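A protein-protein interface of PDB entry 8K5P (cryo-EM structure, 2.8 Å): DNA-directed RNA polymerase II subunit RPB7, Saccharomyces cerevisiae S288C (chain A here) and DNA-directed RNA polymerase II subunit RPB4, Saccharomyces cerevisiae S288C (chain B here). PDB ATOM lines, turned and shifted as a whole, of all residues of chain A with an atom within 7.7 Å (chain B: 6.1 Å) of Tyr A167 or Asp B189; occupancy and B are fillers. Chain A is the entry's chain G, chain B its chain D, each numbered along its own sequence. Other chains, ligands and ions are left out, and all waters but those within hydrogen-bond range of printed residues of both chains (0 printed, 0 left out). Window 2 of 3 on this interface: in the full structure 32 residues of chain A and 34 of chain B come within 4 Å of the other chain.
Hydrophobic or aromatic side chains of chain B that line the printed part of chain A: Leu B194.
Hydrophobic or aromatic side chains of chain A within 4 Å of the printed part of chain B: Val A86, Tyr A167 and Leu A168.
Among the printed residues, Asp or Glu carboxylates within 4 Å of a Lys or Arg side-chain nitrogen of the other chain: Arg A144 with Glu B190 (3.5 Å).
Printed residues of chain B within 4 Å of Val A86: Leu B194.
Ile A163 touches none of the printed residues of chain B.
Of chain B, only Asp B189 (2.8 Å), Glu B190 (3.3 Å), Thr B193 (3.6 Å) and Leu B194 (3.9 Å) come within 4 Å of Tyr A167.
Of the printed residues of chain B, Leu A168 touches Leu B194 (3.9 Å).
Cys B185 touches none of the printed residues of chain A.
Ala B188 touches none of the printed residues of chain A.
Of chain A, only Tyr A167 (2.8 Å) comes within 4 Å of Asp B189.
Of the printed residues of chain A, Glu B190 touches Arg A144 and Tyr A167.
Of the printed residues of chain A, Leu B194 touches Val A86 (3.5 Å), Arg A144 (3.7 Å), Tyr A167 (3.9 Å) and Leu A168 (3.9 Å).
The nearest residue of chain A that does not touch Asp B189 is Glu A165 (6.4 Å).
Val A86 touches Leu B194.
Leu B194 touches Arg A144.
Tyr A167 touches Glu B190 (CD1 to OE2, 3.3 Å).
Thr B193 touches Tyr A167.
CB of Tyr A167 touches CD2 of Leu B194 (3.9 Å).
Leu B194 touches Leu A168.
The side-chain carboxylate of Asp B189 is in hydrogen-bond range of the side-chain hydroxyl of Tyr A167 (2.8 Å).
OE2 of Glu B190 lies within salt-bridge range of NH2 of Arg A144 (3.5 Å).
The side-chain hydroxyl (OG1) of Thr B187 lies within hydrogen-bond range of the backbone NH (N) of Glu B190 (2.9 Å).
O of Gly A169 is in hydrogen-bond range of N of Arg A144, 3.0 Å away.
The side-chain hydroxyl (OG1) of Thr B193 lies within hydrogen-bond range of the backbone carbonyl oxygen (O) of Glu B190, 2.9 Å away.
OD1 of Asp B189 is in hydrogen-bond range of OG1 of Thr B187 (2.7 Å).
O of Asp B189 is in hydrogen-bond range of OG1 of Thr B193, 2.7 Å away.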
ATOM      1  N   VAL A  86     -30.837  -0.586   6.626  1.00  0.00           N
ATOM      2  CA  VAL A  86     -30.707   0.573   7.493  1.00  0.00           C
ATOM      3  C   VAL A  86     -30.036   1.694   6.709  1.00  0.00           C
ATOM      4  O   VAL A  86     -29.328   1.463   5.726  1.00  0.00           O
ATOM      5  CB  VAL A  86     -29.925   0.235   8.781  1.00  0.00           C
ATOM      6  CG1 VAL A  86     -28.427   0.422   8.574  1.00  0.00           C
ATOM      7  CG2 VAL A  86     -30.422   1.080   9.942  1.00  0.00           C
ATOM      8  N   VAL A  87     -30.275   2.932   7.142  1.00  0.00           N
ATOM      9  CA  VAL A  87     -29.752   4.104   6.450  1.00  0.00           C
ATOM     10  C   VAL A  87     -29.804   5.277   7.417  1.00  0.00           C
ATOM     11  O   VAL A  87     -30.685   5.357   8.274  1.00  0.00           O
ATOM     12  CB  VAL A  87     -30.556   4.382   5.152  1.00  0.00           C
ATOM     13  CG1 VAL A  87     -32.053   4.339   5.424  1.00  0.00           C
ATOM     14  CG2 VAL A  87     -30.148   5.696   4.514  1.00  0.00           C
ATOM     15  N   ILE A 143     -30.316  10.769  13.153  1.00  0.00           N
ATOM     16  CA  ILE A 143     -31.254   9.673  13.373  1.00  0.00           C
ATOM     17  C   ILE A 143     -30.967   8.577  12.358  1.00  0.00           C
ATOM     18  O   ILE A 143     -30.730   8.851  11.177  1.00  0.00           O
ATOM     19  CB  ILE A 143     -32.717  10.161  13.282  1.00  0.00           C
ATOM     20  CG1 ILE A 143     -33.690   8.979  13.321  1.00  0.00           C
ATOM     21  CG2 ILE A 143     -32.930  10.992  12.026  1.00  0.00           C
ATOM     22  CD1 ILE A 143     -33.856   8.371  14.695  1.00  0.00           C
ATOM     23  N   ARG A 144     -30.983   7.331  12.825  1.00  0.00           N
ATOM     24  CA  ARG A 144     -30.828   6.163  11.968  1.00  0.00           C
ATOM     25  C   ARG A 144     -32.200   5.535  11.760  1.00  0.00           C
ATOM     26  O   ARG A 144     -32.890   5.208  12.731  1.00  0.00           O
ATOM     27  CB  ARG A 144     -29.856   5.157  12.583  1.00  0.00           C
ATOM     28  CG  ARG A 144     -29.330   4.127  11.601  1.00  0.00           C
ATOM     29  CD  ARG A 144     -27.817   4.199  11.481  1.00  0.00           C
ATOM     30  NE  ARG A 144     -27.148   3.671  12.665  1.00  0.00           N
ATOM     31  CZ  ARG A 144     -25.833   3.634  12.828  1.00  0.00           C
ATOM     32  NH1 ARG A 144     -25.009   4.087  11.898  1.00  0.00           N
ATOM     33  NH2 ARG A 144     -25.332   3.127  13.951  1.00  0.00           N
ATOM     34  N   VAL A 145     -32.591   5.369  10.499  1.00  0.00           N
ATOM     35  CA  VAL A 145     -33.932   4.928  10.136  1.00  0.00           C
ATOM     36  C   VAL A 145     -33.826   3.650   9.319  1.00  0.00           C
ATOM     37  O   VAL A 145     -33.001   3.558   8.403  1.00  0.00           O
ATOM     38  CB  VAL A 145     -34.691   6.015   9.352  1.00  0.00           C
ATOM     39  CG1 VAL A 145     -36.127   5.585   9.104  1.00  0.00           C
ATOM     40  CG2 VAL A 145     -34.650   7.336  10.100  1.00  0.00           C
ATOM     41  N   ILE A 163     -38.547   2.933  13.736  1.00  0.00           N
ATOM     42  CA  ILE A 163     -37.628   3.252  14.819  1.00  0.00           C
ATOM     43  C   ILE A 163     -37.544   2.140  15.853  1.00  0.00           C
ATOM     44  O   ILE A 163     -36.856   2.299  16.867  1.00  0.00           O
ATOM     45  CB  ILE A 163     -38.000   4.589  15.494  1.00  0.00           C
ATOM     46  CG1 ILE A 163     -38.612   5.552  14.475  1.00  0.00           C
ATOM     47  CG2 ILE A 163     -36.773   5.248  16.110  1.00  0.00           C
ATOM     48  CD1 ILE A 163     -37.618   6.090  13.463  1.00  0.00           C
ATOM     49  N   LYS A 164     -38.218   1.015  15.627  1.00  0.00           N
ATOM     50  CA  LYS A 164     -38.161  -0.099  16.562  1.00  0.00           C
ATOM     51  C   LYS A 164     -36.761  -0.703  16.592  1.00  0.00           C
ATOM     52  O   LYS A 164     -35.971  -0.555  15.654  1.00  0.00           O
ATOM     53  CB  LYS A 164     -39.189  -1.167  16.186  1.00  0.00           C
ATOM     54  CG  LYS A 164     -39.844  -1.844  17.379  1.00  0.00           C
ATOM     55  CD  LYS A 164     -40.907  -0.957  18.004  1.00  0.00           C
ATOM     56  CE  LYS A 164     -42.112  -0.810  17.089  1.00  0.00           C
ATOM     57  NZ  LYS A 164     -42.594  -2.130  16.594  1.00  0.00           N
ATOM     58  N   GLU A 165     -36.458  -1.379  17.705  1.00  0.00           N
ATOM     59  CA  GLU A 165     -35.163  -2.008  17.963  1.00  0.00           C
ATOM     60  C   GLU A 165     -34.066  -0.966  18.150  1.00  0.00           C
ATOM     61  O   GLU A 165     -34.141   0.139  17.601  1.00  0.00           O
ATOM     62  CB  GLU A 165     -34.796  -2.987  16.840  1.00  0.00           C
ATOM     63  CG  GLU A 165     -33.708  -3.983  17.208  1.00  0.00           C
ATOM     64  CD  GLU A 165     -32.397  -3.697  16.505  1.00  0.00           C
ATOM     65  OE1 GLU A 165     -32.413  -2.971  15.489  1.00  0.00           O
ATOM     66  OE2 GLU A 165     -31.351  -4.198  16.966  1.00  0.00           O
ATOM     67  N   ASP A 166     -33.045  -1.306  18.933  1.00  0.00           N
ATOM     68  CA  ASP A 166     -31.973  -0.369  19.235  1.00  0.00           C
ATOM     69  C   ASP A 166     -31.102  -0.121  17.998  1.00  0.00           C
ATOM     70  O   ASP A 166     -31.296  -0.712  16.932  1.00  0.00           O
ATOM     71  CB  ASP A 166     -31.183  -0.859  20.454  1.00  0.00           C
ATOM     72  CG  ASP A 166     -30.198  -1.987  20.139  1.00  0.00           C
ATOM     73  OD1 ASP A 166     -29.579  -2.492  21.098  1.00  0.00           O
ATOM     74  OD2 ASP A 166     -30.082  -2.429  18.980  1.00  0.00           O
ATOM     75  N   TYR A 167     -30.139   0.789  18.156  1.00  0.00           N
ATOM     76  CA  TYR A 167     -29.263   1.345  17.125  1.00  0.00           C
ATOM     77  C   TYR A 167     -29.998   2.283  16.178  1.00  0.00           C
ATOM     78  O   TYR A 167     -29.350   2.942  15.354  1.00  0.00           O
ATOM     79  CB  TYR A 167     -28.549   0.270  16.290  1.00  0.00           C
ATOM     80  CG  TYR A 167     -27.896  -0.823  17.102  1.00  0.00           C
ATOM     81  CD1 TYR A 167     -27.099  -0.518  18.198  1.00  0.00           C
ATOM     82  CD2 TYR A 167     -28.063  -2.159  16.765  1.00  0.00           C
ATOM     83  CE1 TYR A 167     -26.496  -1.513  18.940  1.00  0.00           C
ATOM     84  CE2 TYR A 167     -27.465  -3.162  17.503  1.00  0.00           C
ATOM     85  CZ  TYR A 167     -26.682  -2.834  18.589  1.00  0.00           C
ATOM     86  OH  TYR A 167     -26.083  -3.828  19.327  1.00  0.00           O
ATOM     87  N   LEU A 168     -31.322   2.370  16.259  1.00  0.00           N
ATOM     88  CA  LEU A 168     -32.101   3.280  15.423  1.00  0.00           C
ATOM     89  C   LEU A 168     -32.407   4.571  16.181  1.00  0.00           C
ATOM     90  O   LEU A 168     -33.555   4.895  16.485  1.00  0.00           O
ATOM     91  CB  LEU A 168     -33.380   2.594  14.951  1.00  0.00           C
ATOM     92  CG  LEU A 168     -33.369   1.981  13.548  1.00  0.00           C
ATOM     93  CD1 LEU A 168     -32.178   1.057  13.357  1.00  0.00           C
ATOM     94  CD2 LEU A 168     -34.667   1.237  13.294  1.00  0.00           C
ATOM     95  N   GLY A 169     -31.352   5.309  16.489  1.00  0.00           N
ATOM     96  CA  GLY A 169     -31.467   6.553  17.232  1.00  0.00           C
ATOM     97  C   GLY A 169     -30.410   7.543  16.804  1.00  0.00           C
ATOM     98  O   GLY A 169     -29.969   7.543  15.650  1.00  0.00           O
ATOM     99  N   ALA A 170     -29.999   8.397  17.743  1.00  0.00           N
ATOM    100  CA  ALA A 170     -29.001   9.417  17.443  1.00  0.00           C
ATOM    101  C   ALA A 170     -27.591   8.833  17.447  1.00  0.00           C
ATOM    102  O   ALA A 170     -26.850   8.971  16.469  1.00  0.00           O
ATOM    103  CB  ALA A 170     -29.110  10.569  18.447  1.00  0.00           C
ATOM    104  N   ILE A 171     -27.215   8.178  18.544  1.00  0.00           N
ATOM    105  CA  ILE A 171     -25.893   7.571  18.710  1.00  0.00           C
ATOM    106  C   ILE A 171     -24.783   8.600  18.514  1.00  0.00           C
ATOM    107  O   ILE A 171     -24.392   9.291  19.455  1.00  0.00           O
ATOM    108  CB  ILE A 171     -25.703   6.375  17.755  1.00  0.00           C
ATOM    109  CG1 ILE A 171     -26.927   5.459  17.798  1.00  0.00           C
ATOM    110  CG2 ILE A 171     -24.443   5.601  18.116  1.00  0.00           C
ATOM    111  CD1 ILE A 171     -26.765   4.184  16.998  1.00  0.00           C
ATOM    112  OXT ILE A 171     -24.248   8.769  17.417  1.00  0.00           O
ATOM    113  N   CYS B 185     -19.752   1.145  12.352  1.00  0.00           N
ATOM    114  CA  CYS B 185     -20.305   0.186  13.294  1.00  0.00           C
ATOM    115  C   CYS B 185     -19.285  -0.123  14.378  1.00  0.00           C
ATOM    116  O   CYS B 185     -18.075   0.001  14.168  1.00  0.00           O
ATOM    117  CB  CYS B 185     -20.729  -1.110  12.594  1.00  0.00           C
ATOM    118  SG  CYS B 185     -21.742  -2.186  13.621  1.00  0.00           S
ATOM    119  N   THR B 187     -20.031  -3.010  17.078  1.00  0.00           N
ATOM    120  CA  THR B 187     -20.090  -4.416  17.450  1.00  0.00           C
ATOM    121  C   THR B 187     -20.519  -5.270  16.263  1.00  0.00           C
ATOM    122  O   THR B 187     -21.169  -4.797  15.327  1.00  0.00           O
ATOM    123  CB  THR B 187     -21.056  -4.636  18.621  1.00  0.00           C
ATOM    124  OG1 THR B 187     -22.336  -5.037  18.118  1.00  0.00           O
ATOM    125  CG2 THR B 187     -21.214  -3.359  19.433  1.00  0.00           C
ATOM    126  N   ALA B 188     -20.139  -6.550  16.317  1.00  0.00           N
ATOM    127  CA  ALA B 188     -20.486  -7.475  15.244  1.00  0.00           C
ATOM    128  C   ALA B 188     -21.992  -7.676  15.148  1.00  0.00           C
ATOM    129  O   ALA B 188     -22.554  -7.700  14.046  1.00  0.00           O
ATOM    130  CB  ALA B 188     -19.779  -8.813  15.458  1.00  0.00           C
ATOM    131  N   ASP B 189     -22.664  -7.827  16.292  1.00  0.00           N
ATOM    132  CA  ASP B 189     -24.114  -7.993  16.275  1.00  0.00           C
ATOM    133  C   ASP B 189     -24.819  -6.748  15.747  1.00  0.00           C
ATOM    134  O   ASP B 189     -25.850  -6.859  15.072  1.00  0.00           O
ATOM    135  CB  ASP B 189     -24.605  -8.421  17.672  1.00  0.00           C
ATOM    136  CG  ASP B 189     -24.948  -7.251  18.615  1.00  0.00           C
ATOM    137  OD1 ASP B 189     -24.789  -6.058  18.285  1.00  0.00           O
ATOM    138  OD2 ASP B 189     -25.399  -7.553  19.740  1.00  0.00           O
ATOM    139  N   GLU B 190     -24.282  -5.563  16.042  1.00  0.00           N
ATOM    140  CA  GLU B 190     -24.844  -4.338  15.483  1.00  0.00           C
ATOM    141  C   GLU B 190     -24.735  -4.328  13.965  1.00  0.00           C
ATOM    142  O   GLU B 190     -25.678  -3.933  13.270  1.00  0.00           O
ATOM    143  CB  GLU B 190     -24.144  -3.119  16.084  1.00  0.00           C
ATOM    144  CG  GLU B 190     -24.722  -1.786  15.636  1.00  0.00           C
ATOM    145  CD  GLU B 190     -24.129  -0.611  16.389  1.00  0.00           C
ATOM    146  OE1 GLU B 190     -23.156  -0.818  17.145  1.00  0.00           O
ATOM    147  OE2 GLU B 190     -24.634   0.519  16.223  1.00  0.00           O
ATOM    148  N   ALA B 191     -23.590  -4.761  13.431  1.00  0.00           N
ATOM    149  CA  ALA B 191     -23.434  -4.845  11.982  1.00  0.00           C
ATOM    150  C   ALA B 191     -24.391  -5.865  11.383  1.00  0.00           C
ATOM    151  O   ALA B 191     -24.975  -5.629  10.318  1.00  0.00           O
ATOM    152  CB  ALA B 191     -21.989  -5.192  11.627  1.00  0.00           C
ATOM    153  N   LYS B 192     -24.559  -7.010  12.047  1.00  0.00           N
ATOM    154  CA  LYS B 192     -25.464  -8.034  11.534  1.00  0.00           C
ATOM    155  C   LYS B 192     -26.907  -7.544  11.518  1.00  0.00           C
ATOM    156  O   LYS B 192     -27.637  -7.774  10.548  1.00  0.00           O
ATOM    157  CB  LYS B 192     -25.340  -9.310  12.368  1.00  0.00           C
ATOM    158  CG  LYS B 192     -23.995 -10.007  12.237  1.00  0.00           C
ATOM    159  CD  LYS B 192     -23.996 -10.998  11.085  1.00  0.00           C
ATOM    160  CE  LYS B 192     -24.937 -12.160  11.357  1.00  0.00           C
ATOM    161  NZ  LYS B 192     -24.528 -12.936  12.560  1.00  0.00           N
ATOM    162  N   THR B 193     -27.337  -6.866  12.586  1.00  0.00           N
ATOM    163  CA  THR B 193     -28.716  -6.394  12.656  1.00  0.00           C
ATOM    164  C   THR B 193     -28.961  -5.246  11.682  1.00  0.00           C
ATOM    165  O   THR B 193     -29.953  -5.245  10.945  1.00  0.00           O
ATOM    166  CB  THR B 193     -29.054  -5.967  14.085  1.00  0.00           C
ATOM    167  OG1 THR B 193     -27.980  -5.181  14.617  1.00  0.00           O
ATOM    168  CG2 THR B 193     -29.268  -7.188  14.968  1.00  0.00           C
ATOM    169  N   LEU B 194     -28.065  -4.255  11.668  1.00  0.00           N
ATOM    170  CA  LEU B 194     -28.231  -3.121  10.765  1.00  0.00           C
ATOM    171  C   LEU B 194     -28.067  -3.541   9.310  1.00  0.00           C
ATOM    172  O   LEU B 194     -28.797  -3.065   8.434  1.00  0.00           O
ATOM    173  CB  LEU B 194     -27.236  -2.016  11.121  1.00  0.00           C
ATOM    174  CG  LEU B 194     -27.468  -1.295  12.451  1.00  0.00           C
ATOM    175  CD1 LEU B 194     -26.620  -0.034  12.533  1.00  0.00           C
ATOM    176  CD2 LEU B 194     -28.941  -0.971  12.646  1.00  0.00           C
